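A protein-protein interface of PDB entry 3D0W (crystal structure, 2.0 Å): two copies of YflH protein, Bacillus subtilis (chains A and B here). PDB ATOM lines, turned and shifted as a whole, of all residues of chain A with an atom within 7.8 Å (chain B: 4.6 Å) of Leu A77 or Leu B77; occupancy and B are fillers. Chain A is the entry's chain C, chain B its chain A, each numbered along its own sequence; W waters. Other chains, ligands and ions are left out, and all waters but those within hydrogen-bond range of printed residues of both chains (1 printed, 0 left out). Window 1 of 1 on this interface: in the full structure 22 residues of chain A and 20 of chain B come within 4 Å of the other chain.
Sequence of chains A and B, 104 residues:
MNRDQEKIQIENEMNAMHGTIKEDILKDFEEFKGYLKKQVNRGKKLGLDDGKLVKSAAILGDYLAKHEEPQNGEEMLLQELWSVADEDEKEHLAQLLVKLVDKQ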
ATOM      1  N   ILE A  25       5.279  31.684 -24.437  1.00  0.00           N
ATOM      2  CA  ILE A  25       4.611  30.436 -24.083  1.00  0.00           C
ATOM      3  C   ILE A  25       3.103  30.626 -24.213  1.00  0.00           C
ATOM      4  O   ILE A  25       2.435  29.871 -24.918  1.00  0.00           O
ATOM      5  CB  ILE A  25       4.920  30.005 -22.628  1.00  0.00           C
ATOM      6  CG1 ILE A  25       6.433  29.923 -22.404  1.00  0.00           C
ATOM      7  CG2 ILE A  25       4.280  28.654 -22.342  1.00  0.00           C
ATOM      8  CD1 ILE A  25       7.153  28.957 -23.325  1.00  0.00           C
ATOM      9  N   PHE A  29       0.168  28.976 -26.846  1.00  0.00           N
ATOM     10  CA  PHE A  29      -0.983  28.235 -26.348  1.00  0.00           C
ATOM     11  C   PHE A  29      -2.295  28.817 -26.856  1.00  0.00           C
ATOM     12  O   PHE A  29      -3.180  28.075 -27.281  1.00  0.00           O
ATOM     13  CB  PHE A  29      -1.017  28.205 -24.815  1.00  0.00           C
ATOM     14  CG  PHE A  29      -2.162  27.401 -24.264  1.00  0.00           C
ATOM     15  CD1 PHE A  29      -2.169  26.013 -24.378  1.00  0.00           C
ATOM     16  CD2 PHE A  29      -3.268  28.031 -23.697  1.00  0.00           C
ATOM     17  CE1 PHE A  29      -3.262  25.264 -23.941  1.00  0.00           C
ATOM     18  CE2 PHE A  29      -4.369  27.289 -23.257  1.00  0.00           C
ATOM     19  CZ  PHE A  29      -4.366  25.906 -23.382  1.00  0.00           C
ATOM     20  N   PHE A  32      -2.699  27.920 -30.362  1.00  0.00           N
ATOM     21  CA  PHE A  32      -2.987  26.497 -30.452  1.00  0.00           C
ATOM     22  C   PHE A  32      -4.458  26.258 -30.135  1.00  0.00           C
ATOM     23  O   PHE A  32      -5.155  25.545 -30.861  1.00  0.00           O
ATOM     24  CB  PHE A  32      -2.114  25.730 -29.457  1.00  0.00           C
ATOM     25  CG  PHE A  32      -2.516  24.295 -29.269  1.00  0.00           C
ATOM     26  CD1 PHE A  32      -2.315  23.359 -30.277  1.00  0.00           C
ATOM     27  CD2 PHE A  32      -3.104  23.882 -28.078  1.00  0.00           C
ATOM     28  CE1 PHE A  32      -2.695  22.026 -30.099  1.00  0.00           C
ATOM     29  CE2 PHE A  32      -3.488  22.549 -27.888  1.00  0.00           C
ATOM     30  CZ  PHE A  32      -3.280  21.624 -28.902  1.00  0.00           C
ATOM     31  N   LEU A  36      -7.688  24.934 -32.537  1.00  0.00           N
ATOM     32  CA  LEU A  36      -8.579  23.825 -32.214  1.00  0.00           C
ATOM     33  C   LEU A  36     -10.029  24.296 -32.160  1.00  0.00           C
ATOM     34  O   LEU A  36     -10.929  23.595 -32.624  1.00  0.00           O
ATOM     35  CB  LEU A  36      -8.189  23.178 -30.878  1.00  0.00           C
ATOM     36  CG  LEU A  36      -6.836  22.457 -30.834  1.00  0.00           C
ATOM     37  CD1 LEU A  36      -6.710  21.670 -29.535  1.00  0.00           C
ATOM     38  CD2 LEU A  36      -6.706  21.520 -32.019  1.00  0.00           C
ATOM     39  N   LEU A  64      -6.518  14.823 -34.730  1.00  0.00           N
ATOM     40  CA  LEU A  64      -5.326  14.130 -34.255  1.00  0.00           C
ATOM     41  C   LEU A  64      -4.975  12.949 -35.158  1.00  0.00           C
ATOM     42  O   LEU A  64      -3.798  12.661 -35.388  1.00  0.00           O
ATOM     43  CB  LEU A  64      -5.523  13.658 -32.807  1.00  0.00           C
ATOM     44  CG  LEU A  64      -5.688  14.810 -31.801  1.00  0.00           C
ATOM     45  CD1 LEU A  64      -6.070  14.292 -30.432  1.00  0.00           C
ATOM     46  CD2 LEU A  64      -4.390  15.597 -31.731  1.00  0.00           C
ATOM     47  N   PRO A  70       3.810  18.689 -36.203  1.00  0.00           N
ATOM     48  CA  PRO A  70       3.762  19.522 -34.995  1.00  0.00           C
ATOM     49  C   PRO A  70       4.543  20.819 -35.211  1.00  0.00           C
ATOM     50  O   PRO A  70       5.687  20.787 -35.664  1.00  0.00           O
ATOM     51  CB  PRO A  70       4.407  18.632 -33.938  1.00  0.00           C
ATOM     52  CG  PRO A  70       4.052  17.247 -34.406  1.00  0.00           C
ATOM     53  CD  PRO A  70       4.300  17.336 -35.891  1.00  0.00           C
ATOM     54  N   ASN A  72       4.535  23.286 -32.615  1.00  0.00           N
ATOM     55  CA  ASN A  72       4.875  23.773 -31.283  1.00  0.00           C
ATOM     56  C   ASN A  72       4.843  22.606 -30.298  1.00  0.00           C
ATOM     57  O   ASN A  72       4.425  21.501 -30.652  1.00  0.00           O
ATOM     58  CB  ASN A  72       3.882  24.858 -30.850  1.00  0.00           C
ATOM     59  CG  ASN A  72       2.430  24.436 -31.049  1.00  0.00           C
ATOM     60  OD1 ASN A  72       2.003  23.384 -30.572  1.00  0.00           O
ATOM     61  ND2 ASN A  72       1.668  25.259 -31.759  1.00  0.00           N
ATOM     62  N   GLY A  73       5.292  22.861 -29.071  1.00  0.00           N
ATOM     63  CA  GLY A  73       5.317  21.834 -28.041  1.00  0.00           C
ATOM     64  C   GLY A  73       3.954  21.241 -27.725  1.00  0.00           C
ATOM     65  O   GLY A  73       3.858  20.063 -27.370  1.00  0.00           O
ATOM     66  N   GLU A  74       2.901  22.049 -27.841  1.00  0.00           N
ATOM     67  CA  GLU A  74       1.545  21.563 -27.574  1.00  0.00           C
ATOM     68  C   GLU A  74       1.175  20.442 -28.551  1.00  0.00           C
ATOM     69  O   GLU A  74       0.730  19.367 -28.147  1.00  0.00           O
ATOM     70  CB  GLU A  74       0.518  22.700 -27.700  1.00  0.00           C
ATOM     71  CG  GLU A  74       0.472  23.664 -26.520  1.00  0.00           C
ATOM     72  CD  GLU A  74       1.481  24.805 -26.615  1.00  0.00           C
ATOM     73  OE1 GLU A  74       2.296  24.838 -27.561  1.00  0.00           O
ATOM     74  OE2 GLU A  74       1.447  25.677 -25.730  1.00  0.00           O
ATOM     75  N   GLU A  75       1.369  20.693 -29.834  1.00  0.00           N
ATOM     76  CA  GLU A  75       1.045  19.710 -30.849  1.00  0.00           C
ATOM     77  C   GLU A  75       1.984  18.514 -30.815  1.00  0.00           C
ATOM     78  O   GLU A  75       1.580  17.384 -31.120  1.00  0.00           O
ATOM     79  CB  GLU A  75       1.051  20.376 -32.227  1.00  0.00           C
ATOM     80  CG  GLU A  75      -0.111  21.337 -32.418  1.00  0.00           C
ATOM     81  CD  GLU A  75       0.100  22.330 -33.550  1.00  0.00           C
ATOM     82  OE1 GLU A  75       0.949  22.083 -34.436  1.00  0.00           O
ATOM     83  OE2 GLU A  75      -0.603  23.363 -33.557  1.00  0.00           O
ATOM     84  N   MET A  76       3.236  18.758 -30.445  1.00  0.00           N
ATOM     85  CA  MET A  76       4.217  17.688 -30.352  1.00  0.00           C
ATOM     86  C   MET A  76       3.786  16.742 -29.225  1.00  0.00           C
ATOM     87  O   MET A  76       3.807  15.518 -29.383  1.00  0.00           O
ATOM     88  CB  MET A  76       5.603  18.274 -30.060  1.00  0.00           C
ATOM     89  CG  MET A  76       6.735  17.260 -30.049  1.00  0.00           C
ATOM     90  SD  MET A  76       6.931  16.348 -31.746  1.00  0.00           S
ATOM     91  CE  MET A  76       7.625  14.667 -31.094  1.00  0.00           C
ATOM     92  N   LEU A  77       3.389  17.306 -28.087  1.00  0.00           N
ATOM     93  CA  LEU A  77       2.960  16.471 -26.968  1.00  0.00           C
ATOM     94  C   LEU A  77       1.691  15.699 -27.316  1.00  0.00           C
ATOM     95  O   LEU A  77       1.597  14.508 -27.035  1.00  0.00           O
ATOM     96  CB  LEU A  77       2.703  17.309 -25.711  1.00  0.00           C
ATOM     97  CG  LEU A  77       2.157  16.504 -24.516  1.00  0.00           C
ATOM     98  CD1 LEU A  77       3.191  15.470 -24.066  1.00  0.00           C
ATOM     99  CD2 LEU A  77       1.811  17.448 -23.370  1.00  0.00           C
ATOM    100  N   LEU A  78       0.713  16.373 -27.912  1.00  0.00           N
ATOM    101  CA  LEU A  78      -0.537  15.704 -28.280  1.00  0.00           C
ATOM    102  C   LEU A  78      -0.303  14.537 -29.232  1.00  0.00           C
ATOM    103  O   LEU A  78      -0.882  13.468 -29.062  1.00  0.00           O
ATOM    104  CB  LEU A  78      -1.510  16.680 -28.937  1.00  0.00           C
ATOM    105  CG  LEU A  78      -2.529  17.377 -28.040  1.00  0.00           C
ATOM    106  CD1 LEU A  78      -3.383  18.321 -28.890  1.00  0.00           C
ATOM    107  CD2 LEU A  78      -3.407  16.331 -27.357  1.00  0.00           C
ATOM    108  N   GLN A  79       0.534  14.747 -30.245  1.00  0.00           N
ATOM    109  CA  GLN A  79       0.810  13.679 -31.199  1.00  0.00           C
ATOM    110  C   GLN A  79       1.542  12.513 -30.545  1.00  0.00           C
ATOM    111  O   GLN A  79       1.316  11.357 -30.911  1.00  0.00           O
ATOM    112  CB  GLN A  79       1.616  14.206 -32.388  1.00  0.00           C
ATOM    113  CG  GLN A  79       0.829  15.145 -33.299  1.00  0.00           C
ATOM    114  CD  GLN A  79      -0.350  14.455 -33.981  1.00  0.00           C
ATOM    115  OE1 GLN A  79      -0.211  13.354 -34.522  1.00  0.00           O
ATOM    116  NE2 GLN A  79      -1.507  15.103 -33.965  1.00  0.00           N
ATOM    117  N   GLU A  80       2.426  12.802 -29.591  1.00  0.00           N
ATOM    118  CA  GLU A  80       3.141  11.725 -28.908  1.00  0.00           C
ATOM    119  C   GLU A  80       2.179  10.967 -27.989  1.00  0.00           C
ATOM    120  O   GLU A  80       2.231   9.744 -27.908  1.00  0.00           O
ATOM    121  CB  GLU A  80       4.325  12.273 -28.095  1.00  0.00           C
ATOM    122  CG  GLU A  80       5.533  12.704 -28.941  1.00  0.00           C
ATOM    123  CD  GLU A  80       6.249  11.528 -29.593  1.00  0.00           C
ATOM    124  OE1 GLU A  80       6.450  10.497 -28.917  1.00  0.00           O
ATOM    125  OE2 GLU A  80       6.623  11.638 -30.779  1.00  0.00           O
ATOM    126  N   LEU A  81       1.302  11.687 -27.293  1.00  0.00           N
ATOM    127  CA  LEU A  81       0.340  11.023 -26.408  1.00  0.00           C
ATOM    128  C   LEU A  81      -0.576  10.130 -27.241  1.00  0.00           C
ATOM    129  O   LEU A  81      -0.874   8.994 -26.860  1.00  0.00           O
ATOM    130  CB  LEU A  81      -0.514  12.051 -25.654  1.00  0.00           C
ATOM    131  CG  LEU A  81       0.130  12.812 -24.486  1.00  0.00           C
ATOM    132  CD1 LEU A  81      -0.837  13.884 -23.961  1.00  0.00           C
ATOM    133  CD2 LEU A  81       0.491  11.834 -23.379  1.00  0.00           C
ATOM    134  N   TRP A  82      -1.022  10.658 -28.375  1.00  0.00           N
ATOM    135  CA  TRP A  82      -1.906   9.922 -29.272  1.00  0.00           C
ATOM    136  C   TRP A  82      -1.234   8.628 -29.743  1.00  0.00           C
ATOM    137  O   TRP A  82      -1.865   7.576 -29.777  1.00  0.00           O
ATOM    138  CB  TRP A  82      -2.262  10.793 -30.480  1.00  0.00           C
ATOM    139  CG  TRP A  82      -3.498  10.362 -31.234  1.00  0.00           C
ATOM    140  CD1 TRP A  82      -3.548   9.797 -32.477  1.00  0.00           C
ATOM    141  CD2 TRP A  82      -4.863  10.541 -30.820  1.00  0.00           C
ATOM    142  NE1 TRP A  82      -4.859   9.624 -32.867  1.00  0.00           N
ATOM    143  CE2 TRP A  82      -5.685  10.071 -31.869  1.00  0.00           C
ATOM    144  CE3 TRP A  82      -5.469  11.059 -29.666  1.00  0.00           C
ATOM    145  CZ2 TRP A  82      -7.088  10.103 -31.803  1.00  0.00           C
ATOM    146  CZ3 TRP A  82      -6.868  11.093 -29.598  1.00  0.00           C
ATOM    147  CH2 TRP A  82      -7.657  10.614 -30.665  1.00  0.00           C
ATOM    148  N   SER A  83       0.049   8.707 -30.084  1.00  0.00           N
ATOM    149  CA  SER A  83       0.789   7.533 -30.562  1.00  0.00           C
ATOM    150  C   SER A  83       0.961   6.379 -29.564  1.00  0.00           C
ATOM    151  O   SER A  83       1.311   5.266 -29.962  1.00  0.00           O
ATOM    152  CB  SER A  83       2.174   7.956 -31.073  1.00  0.00           C
ATOM    153  OG  SER A  83       3.041   8.257 -29.992  1.00  0.00           O
ATOM    154  N   VAL A  84       0.758   6.619 -28.272  1.00  0.00           N
ATOM    155  CA  VAL A  84       0.891   5.525 -27.303  1.00  0.00           C
ATOM    156  C   VAL A  84      -0.431   5.159 -26.639  1.00  0.00           C
ATOM    157  O   VAL A  84      -0.467   4.322 -25.737  1.00  0.00           O
ATOM    158  CB  VAL A  84       1.918   5.840 -26.171  1.00  0.00           C
ATOM    159  CG1 VAL A  84       3.308   5.999 -26.769  1.00  0.00           C
ATOM    160  CG2 VAL A  84       1.501   7.095 -25.393  1.00  0.00           C
ATOM    161  N   LEU A  93      -8.873  11.122 -24.251  1.00  0.00           N
ATOM    162  CA  LEU A  93      -7.957  12.236 -24.452  1.00  0.00           C
ATOM    163  C   LEU A  93      -8.667  13.295 -25.292  1.00  0.00           C
ATOM    164  O   LEU A  93      -8.585  14.489 -25.001  1.00  0.00           O
ATOM    165  CB  LEU A  93      -6.676  11.769 -25.148  1.00  0.00           C
ATOM    166  CG  LEU A  93      -5.637  12.866 -25.413  1.00  0.00           C
ATOM    167  CD1 LEU A  93      -5.301  13.605 -24.113  1.00  0.00           C
ATOM    168  CD2 LEU A  93      -4.392  12.240 -26.025  1.00  0.00           C
ATOM    169  N   LEU A  96     -11.139  15.073 -23.087  1.00  0.00           N
ATOM    170  CA  LEU A  96     -10.442  15.981 -22.179  1.00  0.00           C
ATOM    171  C   LEU A  96      -9.998  17.240 -22.934  1.00  0.00           C
ATOM    172  O   LEU A  96     -10.076  18.359 -22.407  1.00  0.00           O
ATOM    173  CB  LEU A  96      -9.218  15.279 -21.585  1.00  0.00           C
ATOM    174  CG  LEU A  96      -8.433  16.000 -20.498  1.00  0.00           C
ATOM    175  CD1 LEU A  96      -9.379  16.383 -19.369  1.00  0.00           C
ATOM    176  CD2 LEU A  96      -7.328  15.083 -19.981  1.00  0.00           C
ATOM    177  N   LEU A  97      -9.520  17.048 -24.160  1.00  0.00           N
ATOM    178  CA  LEU A  97      -9.062  18.155 -24.994  1.00  0.00           C
ATOM    179  C   LEU A  97     -10.215  19.116 -25.307  1.00  0.00           C
ATOM    180  O   LEU A  97     -10.013  20.329 -25.429  1.00  0.00           O
ATOM    181  CB  LEU A  97      -8.451  17.622 -26.301  1.00  0.00           C
ATOM    182  CG  LEU A  97      -7.761  18.628 -27.233  1.00  0.00           C
ATOM    183  CD1 LEU A  97      -6.596  19.285 -26.491  1.00  0.00           C
ATOM    184  CD2 LEU A  97      -7.249  17.921 -28.494  1.00  0.00           C
ATOM    185  N   LEU A 100     -10.585  21.361 -22.512  1.00  0.00           N
ATOM    186  CA  LEU A 100      -9.488  22.324 -22.513  1.00  0.00           C
ATOM    187  C   LEU A 100      -9.841  23.449 -23.487  1.00  0.00           C
ATOM    188  O   LEU A 100      -9.715  24.628 -23.169  1.00  0.00           O
ATOM    189  CB  LEU A 100      -8.171  21.655 -22.944  1.00  0.00           C
ATOM    190  CG  LEU A 100      -6.958  22.583 -23.122  1.00  0.00           C
ATOM    191  CD1 LEU A 100      -5.690  21.833 -22.773  1.00  0.00           C
ATOM    192  CD2 LEU A 100      -6.901  23.119 -24.544  1.00  0.00           C
ATOM    193  N   PHE B  29      11.153  18.318 -27.115  1.00  0.00           N
ATOM    194  CA  PHE B  29      10.346  17.212 -26.613  1.00  0.00           C
ATOM    195  C   PHE B  29      11.245  16.189 -25.937  1.00  0.00           C
ATOM    196  O   PHE B  29      10.919  15.672 -24.867  1.00  0.00           O
ATOM    197  CB  PHE B  29       9.570  16.526 -27.736  1.00  0.00           C
ATOM    198  CG  PHE B  29       8.778  15.337 -27.265  1.00  0.00           C
ATOM    199  CD1 PHE B  29       7.608  15.512 -26.534  1.00  0.00           C
ATOM    200  CD2 PHE B  29       9.249  14.043 -27.476  1.00  0.00           C
ATOM    201  CE1 PHE B  29       6.913  14.408 -26.011  1.00  0.00           C
ATOM    202  CE2 PHE B  29       8.571  12.936 -26.962  1.00  0.00           C
ATOM    203  CZ  PHE B  29       7.403  13.115 -26.227  1.00  0.00           C
ATOM    204  N   PHE B  32      12.063  17.428 -22.622  1.00  0.00           N
ATOM    205  CA  PHE B  32      10.864  17.368 -21.790  1.00  0.00           C
ATOM    206  C   PHE B  32      10.697  15.937 -21.280  1.00  0.00           C
ATOM    207  O   PHE B  32      10.540  15.696 -20.085  1.00  0.00           O
ATOM    208  CB  PHE B  32       9.641  17.775 -22.619  1.00  0.00           C
ATOM    209  CG  PHE B  32       8.327  17.393 -21.996  1.00  0.00           C
ATOM    210  CD1 PHE B  32       7.904  17.983 -20.808  1.00  0.00           C
ATOM    211  CD2 PHE B  32       7.514  16.435 -22.594  1.00  0.00           C
ATOM    212  CE1 PHE B  32       6.690  17.624 -20.227  1.00  0.00           C
ATOM    213  CE2 PHE B  32       6.300  16.070 -22.021  1.00  0.00           C
ATOM    214  CZ  PHE B  32       5.887  16.668 -20.832  1.00  0.00           C
ATOM    215  N   GLY B  73       5.865  24.465 -24.471  1.00  0.00           N
ATOM    216  CA  GLY B  73       4.536  24.079 -24.925  1.00  0.00           C
ATOM    217  C   GLY B  73       4.043  22.762 -24.352  1.00  0.00           C
ATOM    218  O   GLY B  73       2.849  22.603 -24.095  1.00  0.00           O
ATOM    219  N   GLU B  74       4.956  21.814 -24.165  1.00  0.00           N
ATOM    220  CA  GLU B  74       4.603  20.516 -23.614  1.00  0.00           C
ATOM    221  C   GLU B  74       4.001  20.696 -22.221  1.00  0.00           C
ATOM    222  O   GLU B  74       2.905  20.203 -21.919  1.00  0.00           O
ATOM    223  CB  GLU B  74       5.841  19.610 -23.518  1.00  0.00           C
ATOM    224  CG  GLU B  74       6.287  18.981 -24.839  1.00  0.00           C
ATOM    225  CD  GLU B  74       7.146  19.895 -25.703  1.00  0.00           C
ATOM    226  OE1 GLU B  74       7.284  21.098 -25.380  1.00  0.00           O
ATOM    227  OE2 GLU B  74       7.681  19.400 -26.718  1.00  0.00           O
ATOM    228  N   GLU B  75       4.722  21.424 -21.379  1.00  0.00           N
ATOM    229  CA  GLU B  75       4.288  21.654 -20.009  1.00  0.00           C
ATOM    230  C   GLU B  75       3.034  22.506 -19.912  1.00  0.00           C
ATOM    231  O   GLU B  75       2.203  22.308 -19.019  1.00  0.00           O
ATOM    232  CB  GLU B  75       5.433  22.279 -19.220  1.00  0.00           C
ATOM    233  CG  GLU B  75       6.547  21.273 -18.953  1.00  0.00           C
ATOM    234  CD  GLU B  75       7.819  21.916 -18.425  1.00  0.00           C
ATOM    235  OE1 GLU B  75       7.760  23.062 -17.923  1.00  0.00           O
ATOM    236  OE2 GLU B  75       8.876  21.260 -18.503  1.00  0.00           O
ATOM    237  N   MET B  76       2.902  23.452 -20.830  1.00  0.00           N
ATOM    238  CA  MET B  76       1.738  24.318 -20.850  1.00  0.00           C
ATOM    239  C   MET B  76       0.495  23.477 -21.155  1.00  0.00           C
ATOM    240  O   MET B  76      -0.519  23.586 -20.468  1.00  0.00           O
ATOM    241  CB  MET B  76       1.900  25.398 -21.911  1.00  0.00           C
ATOM    242  CG  MET B  76       0.744  26.354 -21.955  1.00  0.00           C
ATOM    243  SD  MET B  76       0.581  27.347 -20.296  1.00  0.00           S
ATOM    244  CE  MET B  76       0.653  29.104 -21.085  1.00  0.00           C
ATOM    245  N   LEU B  77       0.569  22.637 -22.184  1.00  0.00           N
ATOM    246  CA  LEU B  77      -0.575  21.788 -22.523  1.00  0.00           C
ATOM    247  C   LEU B  77      -0.910  20.849 -21.358  1.00  0.00           C
ATOM    248  O   LEU B  77      -2.076  20.700 -20.993  1.00  0.00           O
ATOM    249  CB  LEU B  77      -0.288  20.966 -23.788  1.00  0.00           C
ATOM    250  CG  LEU B  77      -1.402  20.007 -24.251  1.00  0.00           C
ATOM    251  CD1 LEU B  77      -2.648  20.800 -24.559  1.00  0.00           C
ATOM    252  CD2 LEU B  77      -0.957  19.240 -25.502  1.00  0.00           C
ATOM    253  N   LEU B  78       0.104  20.222 -20.761  1.00  0.00           N
ATOM    254  CA  LEU B  78      -0.143  19.308 -19.655  1.00  0.00           C
ATOM    255  C   LEU B  78      -0.865  19.961 -18.493  1.00  0.00           C
ATOM    256  O   LEU B  78      -1.814  19.389 -17.948  1.00  0.00           O
ATOM    257  CB  LEU B  78       1.155  18.697 -19.127  1.00  0.00           C
ATOM    258  CG  LEU B  78       1.650  17.423 -19.798  1.00  0.00           C
ATOM    259  CD1 LEU B  78       2.892  16.921 -19.059  1.00  0.00           C
ATOM    260  CD2 LEU B  78       0.530  16.359 -19.766  1.00  0.00           C
ATOM    261  N   GLN B  79      -0.413  21.145 -18.101  1.00  0.00           N
ATOM    262  CA  GLN B  79      -1.042  21.836 -16.979  1.00  0.00           C
ATOM    263  C   GLN B  79      -2.474  22.253 -17.299  1.00  0.00           C
ATOM    264  O   GLN B  79      -3.343  22.189 -16.435  1.00  0.00           O
ATOM    265  CB  GLN B  79      -0.228  23.064 -16.566  1.00  0.00           C
ATOM    266  CG  GLN B  79       1.077  22.738 -15.845  1.00  0.00           C
ATOM    267  CD  GLN B  79       0.883  21.901 -14.580  1.00  0.00           C
ATOM    268  OE1 GLN B  79      -0.072  22.093 -13.823  1.00  0.00           O
ATOM    269  NE2 GLN B  79       1.807  20.978 -14.341  1.00  0.00           N
ATOM    270  N   GLU B  80      -2.712  22.691 -18.529  1.00  0.00           N
ATOM    271  CA  GLU B  80      -4.055  23.099 -18.938  1.00  0.00           C
ATOM    272  C   GLU B  80      -4.996  21.884 -18.958  1.00  0.00           C
ATOM    273  O   GLU B  80      -6.158  21.987 -18.572  1.00  0.00           O
ATOM    274  CB  GLU B  80      -4.019  23.760 -20.313  1.00  0.00           C
ATOM    275  CG  GLU B  80      -3.469  25.181 -20.319  1.00  0.00           C
ATOM    276  CD  GLU B  80      -4.291  26.137 -19.468  1.00  0.00           C
ATOM    277  OE1 GLU B  80      -5.540  26.076 -19.516  1.00  0.00           O
ATOM    278  OE2 GLU B  80      -3.689  26.961 -18.754  1.00  0.00           O
ATOM    279  N   LEU B  81      -4.488  20.738 -19.401  1.00  0.00           N
ATOM    280  CA  LEU B  81      -5.285  19.511 -19.424  1.00  0.00           C
ATOM    281  C   LEU B  81      -5.602  19.103 -17.994  1.00  0.00           C
ATOM    282  O   LEU B  81      -6.727  18.734 -17.676  1.00  0.00           O
ATOM    283  CB  LEU B  81      -4.516  18.372 -20.120  1.00  0.00           C
ATOM    284  CG  LEU B  81      -4.473  18.418 -21.653  1.00  0.00           C
ATOM    285  CD1 LEU B  81      -3.477  17.377 -22.206  1.00  0.00           C
ATOM    286  CD2 LEU B  81      -5.875  18.138 -22.190  1.00  0.00           C
ATOM    287  N   LEU B 100       4.201   7.361 -22.491  1.00  0.00           N
ATOM    288  CA  LEU B 100       4.921   8.282 -23.358  1.00  0.00           C
ATOM    289  C   LEU B 100       6.383   8.365 -22.918  1.00  0.00           C
ATOM    290  O   LEU B 100       7.295   8.318 -23.749  1.00  0.00           O
ATOM    291  CB  LEU B 100       4.256   9.662 -23.334  1.00  0.00           C
ATOM    292  CG  LEU B 100       4.943  10.859 -23.995  1.00  0.00           C
ATOM    293  CD1 LEU B 100       3.901  11.896 -24.355  1.00  0.00           C
ATOM    294  CD2 LEU B 100       5.997  11.456 -23.058  1.00  0.00           C
HETATM  295  O   HOH W   1      -7.824  25.984 -21.691  1.00  0.00           O
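Water W1 lies within hydrogen-bond range of O of Leu A100 and OE1 of Glu B80.
Leu A77 touches just these residues of chain B: Phe B32, Glu B74, Leu B77, Leu B78 and Leu B100.
Printed residues of chain B within 4 Å of Ile A25: Met B76 (3.9 Å).
Of the printed residues of chain B, Leu A81 touches Leu B100.
Of the printed residues of chain B, Met A76 touches Phe B29.
Of the printed residues of chain A, Gly B73 touches Gly A73 (3.7 Å) and Glu A74 (3.5 Å).
Printed residues of chain B within 4 Å of Val A84: Leu B100 (3.97 Å).
Leu A36 touches none of the printed residues of chain B.
Ser A83 touches none of the printed residues of chain B.
The nearest printed residue of chain B that does not touch Val A84 is Phe B29 (8.2 Å).
Of the 12 printed residues of chain B, 10 touch a printed residue of chain A.
Hydrophobic or aromatic side chains of chain B that line the printed part of chain A: Phe B29, Phe B32, Met B76, Leu B77, Leu B78, Leu B81 and Leu B100.
Along chain B the printed residues that touch a printed residue of chain A span positions 29 to 100.
Hydrophobic or aromatic side chains of chain A that line the printed part of chain B: Ile A25, Phe A29, Phe A32, Met A76, Leu A77, Leu A78, Leu A81, Val A84, Leu A96 and Leu A100.
Met B76 touches Phe A29.
Gly B73 touches Gly A73 (C to C, 3.7 Å).
Gly A73 touches Glu B74.
Glu A74 touches Leu B77 (O to CD2, 3.1 Å).
CD2 of Leu A77 touches CG of Leu B78 (3.6 Å).
Leu A77 touches Leu B100 (CD1 to CD1, 3.7 Å).
Leu B77 touches Leu A78 (CD2 to CG, 3.5 Å).
Phe B29 touches Glu A80.
Leu A81 touches Leu B100.
Leu B81 touches Leu A100 (N to CD1, 3.7 Å).
Phe A29 touches Met B76, and with the chains exchanged Met A76 touches Phe B29.
Phe A29 touches Glu B80, and with the chains exchanged Glu A80 touches Phe B29.
Glu A74 touches Met B76, but with the chains exchanged Met A76 does not touch Glu B74 (4.1 Å).
Leu A77 touches Leu B100, and with the chains exchanged Leu A100 touches Leu B77.
Positions printed for both chains: 29, 32, 73, 74, 75, 76, 77, 78, 79, 80, 81 and 100.
Of the 24 pairs that touch across the chains among the printed residues, 20 have their exchanged pair printed and touching as well.
OD1 of Asn A72 is in hydrogen-bond range of N of Glu A74 (3.2 Å).
The backbone carbonyl oxygen (O) of Glu A80 sits at hydrogen-bond distance from the side-chain hydroxyl (OG) of Ser A83 (2.7 Å).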
